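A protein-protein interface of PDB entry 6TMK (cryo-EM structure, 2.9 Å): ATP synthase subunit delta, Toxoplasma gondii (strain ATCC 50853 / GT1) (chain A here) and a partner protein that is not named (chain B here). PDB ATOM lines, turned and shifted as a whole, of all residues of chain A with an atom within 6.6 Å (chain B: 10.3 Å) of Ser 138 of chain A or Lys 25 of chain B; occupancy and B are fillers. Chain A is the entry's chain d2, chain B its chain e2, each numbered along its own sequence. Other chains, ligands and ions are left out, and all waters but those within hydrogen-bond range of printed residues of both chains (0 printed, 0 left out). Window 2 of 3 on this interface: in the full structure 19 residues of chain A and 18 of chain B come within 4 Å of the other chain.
The backbone NH (N) of Lys 25 of chain B lies within hydrogen-bond range of the backbone carbonyl oxygen (O) of Met 139 of chain A (3.4 Å). NZ of Lys 25 of chain B lies within hydrogen-bond range of O of Ser 138 of chain A, at 3.3 Å.
OD2 of Asp 141 of chain A sits at hydrogen-bond distance from N of Ser 144 of chain A (2.6 Å). The side-chain sulfur of Cys 23 of chain B sits at hydrogen-bond distance from the backbone carbonyl oxygen of Leu 19 of chain B (2.8 Å). The backbone carbonyl oxygen of Gln 22 of chain B lies within hydrogen-bond range of the guanidinium group of Arg 29 of chain B (2.8 Å).
CG1 of Val 135 of chain A touches CD2 of Leu 24 of chain B (3.6 Å). O of Met 139 of chain A touches CD2 of Leu 24 of chain B, 3.6 Å away. CD2 of Tyr 28 of chain B touches SD of Met 139 of chain A, at 3.5 Å. Leu 140 of chain A touches Cys 23 of chain B (CD2 to O, 3.5 Å). Leu 140 of chain A touches Lys 25 of chain B (O to CE, 3.3 Å). O of Cys 23 of chain B touches N of Asp 141 of chain A, 3.7 Å away. Ser 144 of chain A touches Arg 29 of chain B (OG to NH1, 3.9 Å).
Ser 138 of chain A touches one residue of chain B. Lys 25 of chain B touches just these residues of chain A: Ser 138, Met 139 and Leu 140. No residue of chain B comes within 4 Å of Pro 136 of chain A. Met 139 of chain A touches just these residues of chain B: Leu 24, Lys 25 and Tyr 28. Printed residues of chain A within 4 Å of Leu 24 of chain B: Val 135 and Met 139. Printed residues of chain A within 4 Å of Tyr 28 of chain B: Met 139. Of the printed residues of chain A, Cys 23 of chain B touches Leu 140 and Asp 141. Printed residues of chain A within 4 Å of Arg 29 of chain B: Ser 144. Printed residues of chain B within 4 Å of Val 135 of chain A: Leu 24 (3.6 Å). Arg 21 of chain B touches none of the printed residues of chain A. Leu 19 of chain B touches none of the printed residues of chain A. The nearest residue of chain B that does not touch Ser 138 of chain A is Tyr 28 of chain B (5.8 Å). The nearest printed residue of chain B that does not touch Leu 140 of chain A is Leu 20 of chain B (4.1 Å).
Of the 10 printed residues of chain A, 6 touch a printed residue of chain B. Hydrophobic or aromatic side chains of chain A within 4 Å of the printed part of chain B: Val 135, Met 139 and Leu 140. Hydrophobic or aromatic side chains of chain B within 4 Å of the printed part of chain A: Leu 24 and Tyr 28. Among the printed residues, no Asp or Glu carboxylate lies within 4 Å of a Lys or Arg side-chain nitrogen of the other chain.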
ATOM      1  N   ARG A 105     -17.529  32.202 -17.968  1.00  0.00           N
ATOM      2  CA  ARG A 105     -17.700  31.347 -16.803  1.00  0.00           C
ATOM      3  C   ARG A 105     -16.916  30.056 -16.974  1.00  0.00           C
ATOM      4  O   ARG A 105     -16.922  29.448 -18.049  1.00  0.00           O
ATOM      5  CB  ARG A 105     -19.176  31.016 -16.581  1.00  0.00           C
ATOM      6  CG  ARG A 105     -19.951  32.075 -15.828  1.00  0.00           C
ATOM      7  CD  ARG A 105     -21.373  31.619 -15.558  1.00  0.00           C
ATOM      8  NE  ARG A 105     -22.061  32.490 -14.610  1.00  0.00           N
ATOM      9  CZ  ARG A 105     -22.528  33.698 -14.908  1.00  0.00           C
ATOM     10  NH1 ARG A 105     -22.385  34.188 -16.133  1.00  0.00           N
ATOM     11  NH2 ARG A 105     -23.141  34.420 -13.979  1.00  0.00           N
ATOM     12  N   VAL A 135     -13.300  23.238 -16.424  1.00  0.00           N
ATOM     13  CA  VAL A 135     -14.222  23.101 -17.548  1.00  0.00           C
ATOM     14  C   VAL A 135     -14.932  24.438 -17.726  1.00  0.00           C
ATOM     15  O   VAL A 135     -14.992  25.233 -16.778  1.00  0.00           O
ATOM     16  CB  VAL A 135     -15.225  21.961 -17.315  1.00  0.00           C
ATOM     17  CG1 VAL A 135     -15.972  21.636 -18.596  1.00  0.00           C
ATOM     18  CG2 VAL A 135     -14.514  20.733 -16.787  1.00  0.00           C
ATOM     19  N   PRO A 136     -15.479  24.731 -18.899  1.00  0.00           N
ATOM     20  CA  PRO A 136     -16.512  25.763 -18.995  1.00  0.00           C
ATOM     21  C   PRO A 136     -17.847  25.252 -18.470  1.00  0.00           C
ATOM     22  O   PRO A 136     -18.030  24.068 -18.187  1.00  0.00           O
ATOM     23  CB  PRO A 136     -16.583  26.045 -20.500  1.00  0.00           C
ATOM     24  CG  PRO A 136     -15.238  25.666 -21.005  1.00  0.00           C
ATOM     25  CD  PRO A 136     -14.897  24.436 -20.218  1.00  0.00           C
ATOM     26  N   VAL A 137     -18.793  26.184 -18.343  1.00  0.00           N
ATOM     27  CA  VAL A 137     -20.130  25.813 -17.898  1.00  0.00           C
ATOM     28  C   VAL A 137     -20.979  25.304 -19.053  1.00  0.00           C
ATOM     29  O   VAL A 137     -21.943  24.561 -18.829  1.00  0.00           O
ATOM     30  CB  VAL A 137     -20.816  27.006 -17.215  1.00  0.00           C
ATOM     31  CG1 VAL A 137     -22.235  26.644 -16.805  1.00  0.00           C
ATOM     32  CG2 VAL A 137     -20.003  27.463 -16.018  1.00  0.00           C
ATOM     33  N   SER A 138     -20.639  25.682 -20.286  1.00  0.00           N
ATOM     34  CA  SER A 138     -21.360  25.179 -21.450  1.00  0.00           C
ATOM     35  C   SER A 138     -21.262  23.664 -21.555  1.00  0.00           C
ATOM     36  O   SER A 138     -22.174  23.018 -22.084  1.00  0.00           O
ATOM     37  CB  SER A 138     -20.821  25.838 -22.719  1.00  0.00           C
ATOM     38  OG  SER A 138     -19.406  25.899 -22.697  1.00  0.00           O
ATOM     39  N   MET A 139     -20.170  23.081 -21.060  1.00  0.00           N
ATOM     40  CA  MET A 139     -19.884  21.664 -21.232  1.00  0.00           C
ATOM     41  C   MET A 139     -20.347  20.825 -20.047  1.00  0.00           C
ATOM     42  O   MET A 139     -19.927  19.671 -19.914  1.00  0.00           O
ATOM     43  CB  MET A 139     -18.387  21.460 -21.461  1.00  0.00           C
ATOM     44  CG  MET A 139     -17.785  22.399 -22.491  1.00  0.00           C
ATOM     45  SD  MET A 139     -16.098  21.955 -22.940  1.00  0.00           S
ATOM     46  CE  MET A 139     -15.715  23.240 -24.126  1.00  0.00           C
ATOM     47  N   LEU A 140     -21.197  21.374 -19.188  1.00  0.00           N
ATOM     48  CA  LEU A 140     -21.644  20.676 -17.992  1.00  0.00           C
ATOM     49  C   LEU A 140     -23.049  20.126 -18.194  1.00  0.00           C
ATOM     50  O   LEU A 140     -23.796  20.563 -19.074  1.00  0.00           O
ATOM     51  CB  LEU A 140     -21.620  21.610 -16.780  1.00  0.00           C
ATOM     52  CG  LEU A 140     -20.285  21.733 -16.047  1.00  0.00           C
ATOM     53  CD1 LEU A 140     -20.335  22.864 -15.037  1.00  0.00           C
ATOM     54  CD2 LEU A 140     -19.925  20.428 -15.362  1.00  0.00           C
ATOM     55  N   ASP A 141     -23.405  19.156 -17.356  1.00  0.00           N
ATOM     56  CA  ASP A 141     -24.694  18.487 -17.436  1.00  0.00           C
ATOM     57  C   ASP A 141     -25.248  18.294 -16.034  1.00  0.00           C
ATOM     58  O   ASP A 141     -24.495  18.025 -15.095  1.00  0.00           O
ATOM     59  CB  ASP A 141     -24.580  17.132 -18.145  1.00  0.00           C
ATOM     60  CG  ASP A 141     -25.818  16.276 -17.968  1.00  0.00           C
ATOM     61  OD1 ASP A 141     -26.937  16.828 -18.019  1.00  0.00           O
ATOM     62  OD2 ASP A 141     -25.672  15.050 -17.777  1.00  0.00           O
ATOM     63  N   SER A 144     -26.368  13.720 -15.667  1.00  0.00           N
ATOM     64  CA  SER A 144     -25.261  12.872 -15.250  1.00  0.00           C
ATOM     65  C   SER A 144     -24.704  13.340 -13.913  1.00  0.00           C
ATOM     66  O   SER A 144     -24.236  12.523 -13.113  1.00  0.00           O
ATOM     67  CB  SER A 144     -24.166  12.871 -16.316  1.00  0.00           C
ATOM     68  OG  SER A 144     -24.641  12.319 -17.532  1.00  0.00           O
ATOM     69  N   PRO A 183     -26.394  25.638 -16.513  1.00  0.00           N
ATOM     70  CA  PRO A 183     -27.487  26.452 -17.042  1.00  0.00           C
ATOM     71  C   PRO A 183     -28.767  25.653 -17.262  1.00  0.00           C
ATOM     72  O   PRO A 183     -29.857  26.079 -16.879  1.00  0.00           O
ATOM     73  CB  PRO A 183     -26.918  26.953 -18.366  1.00  0.00           C
ATOM     74  CG  PRO A 183     -26.039  25.821 -18.835  1.00  0.00           C
ATOM     75  CD  PRO A 183     -25.601  25.040 -17.602  1.00  0.00           C
ATOM     76  OXT PRO A 183     -28.741  24.560 -17.828  1.00  0.00           O
ATOM     77  N   LEU B  19     -14.830  12.913 -10.187  1.00  0.00           N
ATOM     78  CA  LEU B  19     -16.274  13.121 -10.159  1.00  0.00           C
ATOM     79  C   LEU B  19     -16.688  14.254 -11.090  1.00  0.00           C
ATOM     80  O   LEU B  19     -17.688  14.147 -11.816  1.00  0.00           O
ATOM     81  CB  LEU B  19     -16.733  13.411  -8.732  1.00  0.00           C
ATOM     82  CG  LEU B  19     -16.646  12.246  -7.746  1.00  0.00           C
ATOM     83  CD1 LEU B  19     -16.914  12.731  -6.335  1.00  0.00           C
ATOM     84  CD2 LEU B  19     -17.615  11.137  -8.119  1.00  0.00           C
ATOM     85  N   LEU B  20     -15.918  15.342 -11.106  1.00  0.00           N
ATOM     86  CA  LEU B  20     -16.231  16.421 -12.035  1.00  0.00           C
ATOM     87  C   LEU B  20     -16.196  15.926 -13.475  1.00  0.00           C
ATOM     88  O   LEU B  20     -17.076  16.259 -14.276  1.00  0.00           O
ATOM     89  CB  LEU B  20     -15.253  17.579 -11.843  1.00  0.00           C
ATOM     90  CG  LEU B  20     -15.336  18.702 -12.877  1.00  0.00           C
ATOM     91  CD1 LEU B  20     -16.755  19.224 -12.992  1.00  0.00           C
ATOM     92  CD2 LEU B  20     -14.387  19.827 -12.521  1.00  0.00           C
ATOM     93  N   ARG B  21     -15.187  15.128 -13.822  1.00  0.00           N
ATOM     94  CA  ARG B  21     -15.111  14.574 -15.166  1.00  0.00           C
ATOM     95  C   ARG B  21     -16.284  13.647 -15.449  1.00  0.00           C
ATOM     96  O   ARG B  21     -16.730  13.538 -16.597  1.00  0.00           O
ATOM     97  CB  ARG B  21     -13.791  13.827 -15.333  1.00  0.00           C
ATOM     98  CG  ARG B  21     -12.602  14.733 -15.577  1.00  0.00           C
ATOM     99  CD  ARG B  21     -11.483  13.990 -16.267  1.00  0.00           C
ATOM    100  NE  ARG B  21     -11.058  12.829 -15.492  1.00  0.00           N
ATOM    101  CZ  ARG B  21     -10.206  12.882 -14.474  1.00  0.00           C
ATOM    102  NH1 ARG B  21      -9.690  14.042 -14.093  1.00  0.00           N
ATOM    103  NH2 ARG B  21      -9.878  11.775 -13.827  1.00  0.00           N
ATOM    104  N   GLN B  22     -16.791  12.976 -14.416  1.00  0.00           N
ATOM    105  CA  GLN B  22     -17.987  12.156 -14.562  1.00  0.00           C
ATOM    106  C   GLN B  22     -19.226  13.004 -14.800  1.00  0.00           C
ATOM    107  O   GLN B  22     -20.214  12.502 -15.346  1.00  0.00           O
ATOM    108  CB  GLN B  22     -18.191  11.290 -13.321  1.00  0.00           C
ATOM    109  CG  GLN B  22     -17.383  10.009 -13.315  1.00  0.00           C
ATOM    110  CD  GLN B  22     -17.698   9.134 -12.121  1.00  0.00           C
ATOM    111  OE1 GLN B  22     -18.429   9.539 -11.215  1.00  0.00           O
ATOM    112  NE2 GLN B  22     -17.146   7.928 -12.110  1.00  0.00           N
ATOM    113  N   CYS B  23     -19.189  14.275 -14.400  1.00  0.00           N
ATOM    114  CA  CYS B  23     -20.313  15.183 -14.607  1.00  0.00           C
ATOM    115  C   CYS B  23     -20.195  15.974 -15.905  1.00  0.00           C
ATOM    116  O   CYS B  23     -20.704  17.099 -15.992  1.00  0.00           O
ATOM    117  CB  CYS B  23     -20.447  16.142 -13.425  1.00  0.00           C
ATOM    118  SG  CYS B  23     -20.212  15.393 -11.810  1.00  0.00           S
ATOM    119  N   LEU B  24     -19.535  15.416 -16.913  1.00  0.00           N
ATOM    120  CA  LEU B  24     -19.305  16.081 -18.187  1.00  0.00           C
ATOM    121  C   LEU B  24     -20.307  15.611 -19.236  1.00  0.00           C
ATOM    122  O   LEU B  24     -21.044  14.641 -19.051  1.00  0.00           O
ATOM    123  CB  LEU B  24     -17.880  15.835 -18.679  1.00  0.00           C
ATOM    124  CG  LEU B  24     -16.821  16.781 -18.118  1.00  0.00           C
ATOM    125  CD1 LEU B  24     -15.442  16.181 -18.291  1.00  0.00           C
ATOM    126  CD2 LEU B  24     -16.908  18.136 -18.785  1.00  0.00           C
ATOM    127  N   LYS B  25     -20.322  16.328 -20.356  1.00  0.00           N
ATOM    128  CA  LYS B  25     -21.103  15.948 -21.522  1.00  0.00           C
ATOM    129  C   LYS B  25     -20.319  14.965 -22.385  1.00  0.00           C
ATOM    130  O   LYS B  25     -19.092  15.037 -22.489  1.00  0.00           O
ATOM    131  CB  LYS B  25     -21.478  17.179 -22.349  1.00  0.00           C
ATOM    132  CG  LYS B  25     -22.463  18.109 -21.665  1.00  0.00           C
ATOM    133  CD  LYS B  25     -23.140  19.035 -22.666  1.00  0.00           C
ATOM    134  CE  LYS B  25     -24.459  19.566 -22.135  1.00  0.00           C
ATOM    135  NZ  LYS B  25     -24.684  20.985 -22.527  1.00  0.00           N
ATOM    136  N   GLU B  26     -21.051  14.040 -23.004  1.00  0.00           N
ATOM    137  CA  GLU B  26     -20.422  12.857 -23.584  1.00  0.00           C
ATOM    138  C   GLU B  26     -19.342  13.174 -24.609  1.00  0.00           C
ATOM    139  O   GLU B  26     -18.289  12.512 -24.575  1.00  0.00           O
ATOM    140  CB  GLU B  26     -21.499  11.968 -24.214  1.00  0.00           C
ATOM    141  CG  GLU B  26     -22.019  10.882 -23.291  1.00  0.00           C
ATOM    142  CD  GLU B  26     -21.007   9.777 -23.063  1.00  0.00           C
ATOM    143  OE1 GLU B  26     -20.605   9.567 -21.900  1.00  0.00           O
ATOM    144  OE2 GLU B  26     -20.614   9.119 -24.049  1.00  0.00           O
ATOM    145  N   PRO B  27     -19.504  14.144 -25.512  1.00  0.00           N
ATOM    146  CA  PRO B  27     -18.428  14.398 -26.488  1.00  0.00           C
ATOM    147  C   PRO B  27     -17.130  14.845 -25.845  1.00  0.00           C
ATOM    148  O   PRO B  27     -16.055  14.372 -26.235  1.00  0.00           O
ATOM    149  CB  PRO B  27     -19.024  15.488 -27.394  1.00  0.00           C
ATOM    150  CG  PRO B  27     -20.497  15.472 -27.126  1.00  0.00           C
ATOM    151  CD  PRO B  27     -20.646  15.050 -25.706  1.00  0.00           C
ATOM    152  N   TYR B  28     -17.195  15.748 -24.866  1.00  0.00           N
ATOM    153  CA  TYR B  28     -15.996  16.144 -24.138  1.00  0.00           C
ATOM    154  C   TYR B  28     -15.618  15.137 -23.058  1.00  0.00           C
ATOM    155  O   TYR B  28     -14.431  14.975 -22.761  1.00  0.00           O
ATOM    156  CB  TYR B  28     -16.197  17.528 -23.522  1.00  0.00           C
ATOM    157  CG  TYR B  28     -16.642  18.570 -24.522  1.00  0.00           C
ATOM    158  CD1 TYR B  28     -15.861  18.872 -25.630  1.00  0.00           C
ATOM    159  CD2 TYR B  28     -17.841  19.248 -24.362  1.00  0.00           C
ATOM    160  CE1 TYR B  28     -16.262  19.820 -26.551  1.00  0.00           C
ATOM    161  CE2 TYR B  28     -18.251  20.200 -25.276  1.00  0.00           C
ATOM    162  CZ  TYR B  28     -17.458  20.483 -26.369  1.00  0.00           C
ATOM    163  OH  TYR B  28     -17.860  21.428 -27.282  1.00  0.00           O
ATOM    164  N   ARG B  29     -16.603  14.468 -22.456  1.00  0.00           N
ATOM    165  CA  ARG B  29     -16.301  13.472 -21.433  1.00  0.00           C
ATOM    166  C   ARG B  29     -15.508  12.299 -21.995  1.00  0.00           C
ATOM    167  O   ARG B  29     -14.641  11.743 -21.304  1.00  0.00           O
ATOM    168  CB  ARG B  29     -17.609  12.969 -20.824  1.00  0.00           C
ATOM    169  CG  ARG B  29     -17.459  12.022 -19.656  1.00  0.00           C
ATOM    170  CD  ARG B  29     -18.796  11.833 -18.966  1.00  0.00           C
ATOM    171  NE  ARG B  29     -18.884  10.559 -18.262  1.00  0.00           N
ATOM    172  CZ  ARG B  29     -19.949  10.159 -17.573  1.00  0.00           C
ATOM    173  NH1 ARG B  29     -21.023  10.934 -17.493  1.00  0.00           N
ATOM    174  NH2 ARG B  29     -19.942   8.983 -16.962  1.00  0.00           N
ATOM    175  N   THR B  30     -15.775  11.923 -23.247  1.00  0.00           N
ATOM    176  CA  THR B  30     -14.994  10.874 -23.891  1.00  0.00           C
ATOM    177  C   THR B  30     -13.525  11.256 -23.969  1.00  0.00           C
ATOM    178  O   THR B  30     -12.648  10.491 -23.552  1.00  0.00           O
ATOM    179  CB  THR B  30     -15.549  10.594 -25.288  1.00  0.00           C
ATOM    180  OG1 THR B  30     -15.877  11.832 -25.932  1.00  0.00           O
ATOM    181  CG2 THR B  30     -16.792   9.723 -25.200  1.00  0.00           C
ATOM    182  N   GLN B  31     -13.244  12.479 -24.423  1.00  0.00           N
ATOM    183  CA  GLN B  31     -11.864  12.931 -24.542  1.00  0.00           C
ATOM    184  C   GLN B  31     -11.232  13.138 -23.178  1.00  0.00           C
ATOM    185  O   GLN B  31     -10.021  12.949 -23.020  1.00  0.00           O
ATOM    186  CB  GLN B  31     -11.812  14.230 -25.343  1.00  0.00           C
ATOM    187  CG  GLN B  31     -12.364  14.117 -26.752  1.00  0.00           C
ATOM    188  CD  GLN B  31     -12.390  15.450 -27.472  1.00  0.00           C
ATOM    189  OE1 GLN B  31     -11.740  16.407 -27.052  1.00  0.00           O
ATOM    190  NE2 GLN B  31     -13.152  15.523 -28.556  1.00  0.00           N
ATOM    191  N   ALA B  32     -12.038  13.460 -22.170  1.00  0.00           N
ATOM    192  CA  ALA B  32     -11.499  13.702 -20.838  1.00  0.00           C
ATOM    193  C   ALA B  32     -11.054  12.399 -20.188  1.00  0.00           C
ATOM    194  O   ALA B  32      -9.889  12.251 -19.796  1.00  0.00           O
ATOM    195  CB  ALA B  32     -12.544  14.410 -19.977  1.00  0.00           C
ATOM    196  N   MET B  33     -11.963  11.428 -20.076  1.00  0.00           N
ATOM    197  CA  MET B  33     -11.541  10.142 -19.534  1.00  0.00           C
ATOM    198  C   MET B  33     -10.533   9.440 -20.436  1.00  0.00           C
ATOM    199  O   MET B  33      -9.698   8.673 -19.930  1.00  0.00           O
ATOM    200  CB  MET B  33     -12.763   9.249 -19.318  1.00  0.00           C
ATOM    201  CG  MET B  33     -13.771   9.825 -18.337  1.00  0.00           C
ATOM    202  SD  MET B  33     -13.175   9.846 -16.636  1.00  0.00           S
ATOM    203  CE  MET B  33     -14.686  10.218 -15.751  1.00  0.00           C
ATOM    204  N   GLN B  34     -10.498   9.783 -21.728  1.00  0.00           N
ATOM    205  CA  GLN B  34      -9.426   9.301 -22.587  1.00  0.00           C
ATOM    206  C   GLN B  34      -8.098   9.846 -22.095  1.00  0.00           C
ATOM    207  O   GLN B  34      -7.203   9.088 -21.710  1.00  0.00           O
ATOM    208  CB  GLN B  34      -9.696   9.713 -24.037  1.00  0.00           C
ATOM    209  CG  GLN B  34      -8.489   9.627 -24.959  1.00  0.00           C
ATOM    210  CD  GLN B  34      -7.796   8.281 -24.888  1.00  0.00           C
ATOM    211  OE1 GLN B  34      -8.404   7.274 -24.526  1.00  0.00           O
ATOM    212  NE2 GLN B  34      -6.516   8.256 -25.241  1.00  0.00           N
